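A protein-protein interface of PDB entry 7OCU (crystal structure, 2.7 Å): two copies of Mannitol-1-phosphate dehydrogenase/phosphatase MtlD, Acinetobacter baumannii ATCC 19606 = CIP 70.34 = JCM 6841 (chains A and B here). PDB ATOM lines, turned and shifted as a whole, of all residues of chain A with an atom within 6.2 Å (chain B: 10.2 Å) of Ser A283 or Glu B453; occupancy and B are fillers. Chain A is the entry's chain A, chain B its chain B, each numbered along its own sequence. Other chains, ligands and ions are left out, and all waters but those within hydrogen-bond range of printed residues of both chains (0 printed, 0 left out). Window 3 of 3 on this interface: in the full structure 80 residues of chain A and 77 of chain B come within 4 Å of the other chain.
Of chain B, only Asn B456 (3.4 Å) comes within 4 Å of Asn A282. Ser A283 touches three residues of chain B. Printed residues of chain B within 4 Å of Leu A284: Ile B452. No residue of chain B comes within 4 Å of Arg A286. Of chain B, only Val B470 comes within 4 Å of Glu A287. Printed residues of chain A within 4 Å of Ile B452: Ser A283 and Leu A284. Of chain A, only Ser A283 (2.6 Å) comes within 4 Å of Glu B453. The nearest residue of chain B that does not touch Ser A283 is Asp B454 (4.3 Å). The nearest printed residue of chain A that does not touch Asn B456 is Leu A284 (4.4 Å).
The side-chain hydroxyl (OG) of Ser A283 lies within hydrogen-bond range of the backbone carbonyl oxygen (O) of Glu B453 (2.6 Å). ND2 of Asn B456 is in hydrogen-bond range of OD1 of Asn A282 (3.4 Å).
No position is printed for both chains. Of the 6 pairs that touch across the chains among the printed residues, none has its exchanged pair printed and touching as well.
Of the 16 printed residues of chain B, 4 touch a printed residue of chain A. Along chain B the printed residues that touch a printed residue of chain A span positions 452 to 470. Among the printed residues, no Asp or Glu carboxylate lies within 4 Å of a Lys or Arg side-chain nitrogen of the other chain.
The side-chain amide oxygen (OD1) of Asn A282 is in hydrogen-bond range of the backbone NH (N) of Leu A284 (3.3 Å). OG1 of Thr A280 is in hydrogen-bond range of N of Asn A282, at 3.3 Å. OD1 of Asn A282 lies within hydrogen-bond range of N of Phe A285 (3.3 Å). The backbone carbonyl oxygen (O) of Asp B454 lies close to the side-chain amide oxygen (OD1) of Asn B456, 3.2 Å away.
Ser A283 touches Ile B452. OG of Ser A283 touches ND2 of Asn B456 (3.8 Å). Ile B452 touches Leu A284 (CD1 to CD1, 3.9 Å). O of Glu A287 touches CG1 of Val B470, 3.3 Å away.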
ATOM      1  N   THR A 280     -25.380  -1.153  21.747  1.00  0.00           N
ATOM      2  CA  THR A 280     -25.994   0.204  21.725  1.00  0.00           C
ATOM      3  C   THR A 280     -24.938   1.238  21.319  1.00  0.00           C
ATOM      4  O   THR A 280     -23.742   0.993  21.575  1.00  0.00           O
ATOM      5  CB  THR A 280     -26.618   0.553  23.083  1.00  0.00           C
ATOM      6  OG1 THR A 280     -27.404   1.733  22.916  1.00  0.00           O
ATOM      7  CG2 THR A 280     -25.593   0.768  24.175  1.00  0.00           C
ATOM      8  N   ARG A 281     -25.375   2.345  20.711  1.00  0.00           N
ATOM      9  CA  ARG A 281     -24.522   3.511  20.352  1.00  0.00           C
ATOM     10  C   ARG A 281     -24.582   4.558  21.474  1.00  0.00           C
ATOM     11  O   ARG A 281     -23.704   5.444  21.494  1.00  0.00           O
ATOM     12  CB  ARG A 281     -24.966   4.101  19.010  1.00  0.00           C
ATOM     13  CG  ARG A 281     -24.758   3.162  17.830  1.00  0.00           C
ATOM     14  CD  ARG A 281     -25.088   3.809  16.498  1.00  0.00           C
ATOM     15  NE  ARG A 281     -24.859   2.900  15.382  1.00  0.00           N
ATOM     16  CZ  ARG A 281     -25.668   1.904  15.022  1.00  0.00           C
ATOM     17  NH1 ARG A 281     -25.350   1.143  13.987  1.00  0.00           N
ATOM     18  NH2 ARG A 281     -26.785   1.663  15.689  1.00  0.00           N
ATOM     19  N   ASN A 282     -25.577   4.456  22.365  1.00  0.00           N
ATOM     20  CA  ASN A 282     -25.736   5.323  23.564  1.00  0.00           C
ATOM     21  C   ASN A 282     -24.593   5.018  24.541  1.00  0.00           C
ATOM     22  O   ASN A 282     -24.695   4.018  25.282  1.00  0.00           O
ATOM     23  CB  ASN A 282     -27.118   5.144  24.202  1.00  0.00           C
ATOM     24  CG  ASN A 282     -27.447   6.203  25.236  1.00  0.00           C
ATOM     25  OD1 ASN A 282     -26.568   6.685  25.946  1.00  0.00           O
ATOM     26  ND2 ASN A 282     -28.715   6.565  25.334  1.00  0.00           N
ATOM     27  N   SER A 283     -23.547   5.851  24.528  1.00  0.00           N
ATOM     28  CA  SER A 283     -22.298   5.690  25.320  1.00  0.00           C
ATOM     29  C   SER A 283     -22.599   5.763  26.822  1.00  0.00           C
ATOM     30  O   SER A 283     -21.981   4.989  27.579  1.00  0.00           O
ATOM     31  CB  SER A 283     -21.271   6.717  24.917  1.00  0.00           C
ATOM     32  OG  SER A 283     -21.814   8.027  24.983  1.00  0.00           O
ATOM     33  N   LEU A 284     -23.508   6.657  27.230  1.00  0.00           N
ATOM     34  CA  LEU A 284     -23.914   6.865  28.649  1.00  0.00           C
ATOM     35  C   LEU A 284     -24.497   5.562  29.209  1.00  0.00           C
ATOM     36  O   LEU A 284     -24.118   5.187  30.335  1.00  0.00           O
ATOM     37  CB  LEU A 284     -24.932   8.008  28.724  1.00  0.00           C
ATOM     38  CG  LEU A 284     -25.339   8.446  30.132  1.00  0.00           C
ATOM     39  CD1 LEU A 284     -24.148   9.005  30.898  1.00  0.00           C
ATOM     40  CD2 LEU A 284     -26.461   9.471  30.077  1.00  0.00           C
ATOM     41  N   PHE A 285     -25.381   4.906  28.448  1.00  0.00           N
ATOM     42  CA  PHE A 285     -26.030   3.615  28.803  1.00  0.00           C
ATOM     43  C   PHE A 285     -24.966   2.520  28.949  1.00  0.00           C
ATOM     44  O   PHE A 285     -25.015   1.775  29.946  1.00  0.00           O
ATOM     45  CB  PHE A 285     -27.085   3.227  27.762  1.00  0.00           C
ATOM     46  CG  PHE A 285     -28.484   3.691  28.082  1.00  0.00           C
ATOM     47  CD1 PHE A 285     -28.783   5.042  28.170  1.00  0.00           C
ATOM     48  CD2 PHE A 285     -29.504   2.775  28.297  1.00  0.00           C
ATOM     49  CE1 PHE A 285     -30.070   5.467  28.465  1.00  0.00           C
ATOM     50  CE2 PHE A 285     -30.790   3.202  28.592  1.00  0.00           C
ATOM     51  CZ  PHE A 285     -31.071   4.545  28.676  1.00  0.00           C
ATOM     52  N   ARG A 286     -24.041   2.430  27.986  1.00  0.00           N
ATOM     53  CA  ARG A 286     -22.977   1.390  27.932  1.00  0.00           C
ATOM     54  C   ARG A 286     -22.077   1.505  29.170  1.00  0.00           C
ATOM     55  O   ARG A 286     -21.878   0.479  29.849  1.00  0.00           O
ATOM     56  CB  ARG A 286     -22.152   1.522  26.648  1.00  0.00           C
ATOM     57  CG  ARG A 286     -21.026   0.504  26.526  1.00  0.00           C
ATOM     58  CD  ARG A 286     -20.344   0.512  25.169  1.00  0.00           C
ATOM     59  NE  ARG A 286     -19.672   1.776  24.887  1.00  0.00           N
ATOM     60  CZ  ARG A 286     -20.155   2.761  24.126  1.00  0.00           C
ATOM     61  NH1 ARG A 286     -21.339   2.654  23.544  1.00  0.00           N
ATOM     62  NH2 ARG A 286     -19.440   3.859  23.951  1.00  0.00           N
ATOM     63  N   GLU A 287     -21.563   2.709  29.442  1.00  0.00           N
ATOM     64  CA  GLU A 287     -20.561   2.980  30.508  1.00  0.00           C
ATOM     65  C   GLU A 287     -21.206   2.833  31.894  1.00  0.00           C
ATOM     66  O   GLU A 287     -20.494   2.404  32.823  1.00  0.00           O
ATOM     67  CB  GLU A 287     -19.960   4.376  30.328  1.00  0.00           C
ATOM     68  CG  GLU A 287     -19.145   4.529  29.053  1.00  0.00           C
ATOM     69  CD  GLU A 287     -17.823   3.780  29.026  1.00  0.00           C
ATOM     70  OE1 GLU A 287     -17.390   3.298  30.092  1.00  0.00           O
ATOM     71  OE2 GLU A 287     -17.226   3.682  27.934  1.00  0.00           O
ATOM     72  N   ALA A 288     -22.495   3.169  32.022  1.00  0.00           N
ATOM     73  CA  ALA A 288     -23.261   3.150  33.292  1.00  0.00           C
ATOM     74  C   ALA A 288     -23.531   1.704  33.730  1.00  0.00           C
ATOM     75  O   ALA A 288     -23.288   1.392  34.911  1.00  0.00           O
ATOM     76  CB  ALA A 288     -24.550   3.921  33.136  1.00  0.00           C
ATOM     77  N   GLU B 451     -14.583   7.620  29.504  1.00  0.00           N
ATOM     78  CA  GLU B 451     -14.726   8.573  28.368  1.00  0.00           C
ATOM     79  C   GLU B 451     -16.127   8.436  27.756  1.00  0.00           C
ATOM     80  O   GLU B 451     -16.297   7.593  26.852  1.00  0.00           O
ATOM     81  CB  GLU B 451     -13.647   8.323  27.310  1.00  0.00           C
ATOM     82  CG  GLU B 451     -12.250   8.735  27.746  1.00  0.00           C
ATOM     83  CD  GLU B 451     -11.938  10.219  27.625  1.00  0.00           C
ATOM     84  OE1 GLU B 451     -12.887  11.026  27.561  1.00  0.00           O
ATOM     85  OE2 GLU B 451     -10.740  10.565  27.594  1.00  0.00           O
ATOM     86  N   ILE B 452     -17.085   9.238  28.238  1.00  0.00           N
ATOM     87  CA  ILE B 452     -18.487   9.293  27.725  1.00  0.00           C
ATOM     88  C   ILE B 452     -18.529  10.281  26.552  1.00  0.00           C
ATOM     89  O   ILE B 452     -18.630  11.498  26.805  1.00  0.00           O
ATOM     90  CB  ILE B 452     -19.478   9.668  28.848  1.00  0.00           C
ATOM     91  CG1 ILE B 452     -19.398   8.681  30.016  1.00  0.00           C
ATOM     92  CG2 ILE B 452     -20.897   9.787  28.307  1.00  0.00           C
ATOM     93  CD1 ILE B 452     -20.256   9.054  31.205  1.00  0.00           C
ATOM     94  N   GLU B 453     -18.444   9.764  25.322  1.00  0.00           N
ATOM     95  CA  GLU B 453     -18.421  10.555  24.060  1.00  0.00           C
ATOM     96  C   GLU B 453     -19.856  10.755  23.555  1.00  0.00           C
ATOM     97  O   GLU B 453     -20.786  10.224  24.194  1.00  0.00           O
ATOM     98  CB  GLU B 453     -17.573   9.843  23.002  1.00  0.00           C
ATOM     99  CG  GLU B 453     -16.136   9.600  23.430  1.00  0.00           C
ATOM    100  CD  GLU B 453     -15.256   8.941  22.380  1.00  0.00           C
ATOM    101  OE1 GLU B 453     -15.807   8.384  21.409  1.00  0.00           O
ATOM    102  OE2 GLU B 453     -14.020   8.984  22.536  1.00  0.00           O
ATOM    103  N   ASP B 454     -20.009  11.504  22.456  1.00  0.00           N
ATOM    104  CA  ASP B 454     -21.278  11.698  21.701  1.00  0.00           C
ATOM    105  C   ASP B 454     -22.276  12.492  22.554  1.00  0.00           C
ATOM    106  O   ASP B 454     -22.852  11.910  23.494  1.00  0.00           O
ATOM    107  CB  ASP B 454     -21.863  10.355  21.246  1.00  0.00           C
ATOM    108  CG  ASP B 454     -23.025  10.479  20.274  1.00  0.00           C
ATOM    109  OD1 ASP B 454     -23.945   9.639  20.353  1.00  0.00           O
ATOM    110  OD2 ASP B 454     -22.999  11.406  19.438  1.00  0.00           O
ATOM    111  N   CYS B 455     -22.472  13.774  22.221  1.00  0.00           N
ATOM    112  CA  CYS B 455     -23.466  14.683  22.856  1.00  0.00           C
ATOM    113  C   CYS B 455     -24.882  14.217  22.494  1.00  0.00           C
ATOM    114  O   CYS B 455     -25.470  14.777  21.544  1.00  0.00           O
ATOM    115  CB  CYS B 455     -23.247  16.129  22.421  1.00  0.00           C
ATOM    116  SG  CYS B 455     -21.650  16.807  22.942  1.00  0.00           S
ATOM    117  N   ASN B 456     -25.398  13.225  23.229  1.00  0.00           N
ATOM    118  CA  ASN B 456     -26.716  12.578  22.983  1.00  0.00           C
ATOM    119  C   ASN B 456     -27.782  13.277  23.840  1.00  0.00           C
ATOM    120  O   ASN B 456     -28.095  12.768  24.936  1.00  0.00           O
ATOM    121  CB  ASN B 456     -26.663  11.060  23.207  1.00  0.00           C
ATOM    122  CG  ASN B 456     -25.772  10.635  24.357  1.00  0.00           C
ATOM    123  OD1 ASN B 456     -25.462  11.429  25.242  1.00  0.00           O
ATOM    124  ND2 ASN B 456     -25.353   9.380  24.351  1.00  0.00           N
ATOM    125  N   LYS B 457     -28.301  14.408  23.345  1.00  0.00           N
ATOM    126  CA  LYS B 457     -29.356  15.242  23.988  1.00  0.00           C
ATOM    127  C   LYS B 457     -28.869  15.737  25.358  1.00  0.00           C
ATOM    128  O   LYS B 457     -29.702  15.836  26.283  1.00  0.00           O
ATOM    129  CB  LYS B 457     -30.664  14.451  24.102  1.00  0.00           C
ATOM    130  CG  LYS B 457     -31.208  13.907  22.786  1.00  0.00           C
ATOM    131  CD  LYS B 457     -32.522  13.168  22.935  1.00  0.00           C
ATOM    132  CE  LYS B 457     -33.088  12.693  21.614  1.00  0.00           C
ATOM    133  NZ  LYS B 457     -34.296  11.854  21.806  1.00  0.00           N
ATOM    134  N   LEU B 458     -27.572  16.050  25.472  1.00  0.00           N
ATOM    135  CA  LEU B 458     -26.922  16.574  26.705  1.00  0.00           C
ATOM    136  C   LEU B 458     -25.872  17.624  26.323  1.00  0.00           C
ATOM    137  O   LEU B 458     -25.407  17.605  25.164  1.00  0.00           O
ATOM    138  CB  LEU B 458     -26.276  15.415  27.472  1.00  0.00           C
ATOM    139  CG  LEU B 458     -27.231  14.518  28.259  1.00  0.00           C
ATOM    140  CD1 LEU B 458     -26.524  13.254  28.725  1.00  0.00           C
ATOM    141  CD2 LEU B 458     -27.828  15.261  29.444  1.00  0.00           C
ATOM    142  N   THR B 459     -25.516  18.497  27.270  1.00  0.00           N
ATOM    143  CA  THR B 459     -24.454  19.531  27.130  1.00  0.00           C
ATOM    144  C   THR B 459     -23.095  18.886  27.398  1.00  0.00           C
ATOM    145  O   THR B 459     -23.013  17.913  28.144  1.00  0.00           O
ATOM    146  CB  THR B 459     -24.706  20.716  28.071  1.00  0.00           C
ATOM    147  OG1 THR B 459     -24.716  20.231  29.414  1.00  0.00           O
ATOM    148  CG2 THR B 459     -26.007  21.432  27.781  1.00  0.00           C
ATOM    149  N   PRO B 460     -21.992  19.397  26.798  1.00  0.00           N
ATOM    150  CA  PRO B 460     -20.649  18.882  27.080  1.00  0.00           C
ATOM    151  C   PRO B 460     -20.268  18.909  28.570  1.00  0.00           C
ATOM    152  O   PRO B 460     -19.518  18.046  28.988  1.00  0.00           O
ATOM    153  CB  PRO B 460     -19.724  19.828  26.294  1.00  0.00           C
ATOM    154  CG  PRO B 460     -20.597  20.365  25.182  1.00  0.00           C
ATOM    155  CD  PRO B 460     -21.979  20.471  25.792  1.00  0.00           C
ATOM    156  N   GLN B 462     -22.376  18.597  31.299  1.00  0.00           N
ATOM    157  CA  GLN B 462     -23.097  17.456  31.934  1.00  0.00           C
ATOM    158  C   GLN B 462     -22.387  16.142  31.589  1.00  0.00           C
ATOM    159  O   GLN B 462     -22.239  15.296  32.493  1.00  0.00           O
ATOM    160  CB  GLN B 462     -24.553  17.399  31.464  1.00  0.00           C
ATOM    161  CG  GLN B 462     -25.448  18.452  32.099  1.00  0.00           C
ATOM    162  CD  GLN B 462     -26.862  18.377  31.576  1.00  0.00           C
ATOM    163  OE1 GLN B 462     -27.101  18.397  30.370  1.00  0.00           O
ATOM    164  NE2 GLN B 462     -27.817  18.292  32.488  1.00  0.00           N
ATOM    165  N   LEU B 463     -21.973  15.989  30.326  1.00  0.00           N
ATOM    166  CA  LEU B 463     -21.323  14.766  29.779  1.00  0.00           C
ATOM    167  C   LEU B 463     -19.955  14.564  30.448  1.00  0.00           C
ATOM    168  O   LEU B 463     -19.554  13.397  30.622  1.00  0.00           O
ATOM    169  CB  LEU B 463     -21.183  14.909  28.258  1.00  0.00           C
ATOM    170  CG  LEU B 463     -21.238  13.606  27.462  1.00  0.00           C
ATOM    171  CD1 LEU B 463     -22.657  13.058  27.413  1.00  0.00           C
ATOM    172  CD2 LEU B 463     -20.701  13.809  26.054  1.00  0.00           C
ATOM    173  N   ASN B 464     -19.275  15.660  30.805  1.00  0.00           N
ATOM    174  CA  ASN B 464     -17.953  15.651  31.490  1.00  0.00           C
ATOM    175  C   ASN B 464     -18.152  15.275  32.964  1.00  0.00           C
ATOM    176  O   ASN B 464     -17.348  14.475  33.478  1.00  0.00           O
ATOM    177  CB  ASN B 464     -17.233  16.997  31.344  1.00  0.00           C
ATOM    178  CG  ASN B 464     -15.729  16.900  31.502  1.00  0.00           C
ATOM    179  OD1 ASN B 464     -15.218  15.996  32.161  1.00  0.00           O
ATOM    180  ND2 ASN B 464     -15.008  17.833  30.901  1.00  0.00           N
ATOM    181  N   ALA B 466     -20.734  13.593  34.219  1.00  0.00           N
ATOM    182  CA  ALA B 466     -21.217  12.192  34.163  1.00  0.00           C
ATOM    183  C   ALA B 466     -20.024  11.230  34.101  1.00  0.00           C
ATOM    184  O   ALA B 466     -20.083  10.178  34.766  1.00  0.00           O
ATOM    185  CB  ALA B 466     -22.131  12.007  32.976  1.00  0.00           C
ATOM    186  N   SER B 467     -18.990  11.582  33.329  1.00  0.00           N
ATOM    187  CA  SER B 467     -17.756  10.775  33.127  1.00  0.00           C
ATOM    188  C   SER B 467     -17.047  10.540  34.466  1.00  0.00           C
ATOM    189  O   SER B 467     -16.579   9.406  34.687  1.00  0.00           O
ATOM    190  CB  SER B 467     -16.832  11.429  32.129  1.00  0.00           C
ATOM    191  OG  SER B 467     -17.481  11.614  30.881  1.00  0.00           O
ATOM    192  N   VAL B 470     -19.257   8.061  36.734  1.00  0.00           N
ATOM    193  CA  VAL B 470     -19.204   6.666  36.201  1.00  0.00           C
ATOM    194  C   VAL B 470     -17.809   6.073  36.451  1.00  0.00           C
ATOM    195  O   VAL B 470     -17.735   4.861  36.730  1.00  0.00           O
ATOM    196  CB  VAL B 470     -19.583   6.622  34.706  1.00  0.00           C
ATOM    197  CG1 VAL B 470     -19.292   5.268  34.078  1.00  0.00           C
ATOM    198  CG2 VAL B 470     -21.039   7.005  34.485  1.00  0.00           C
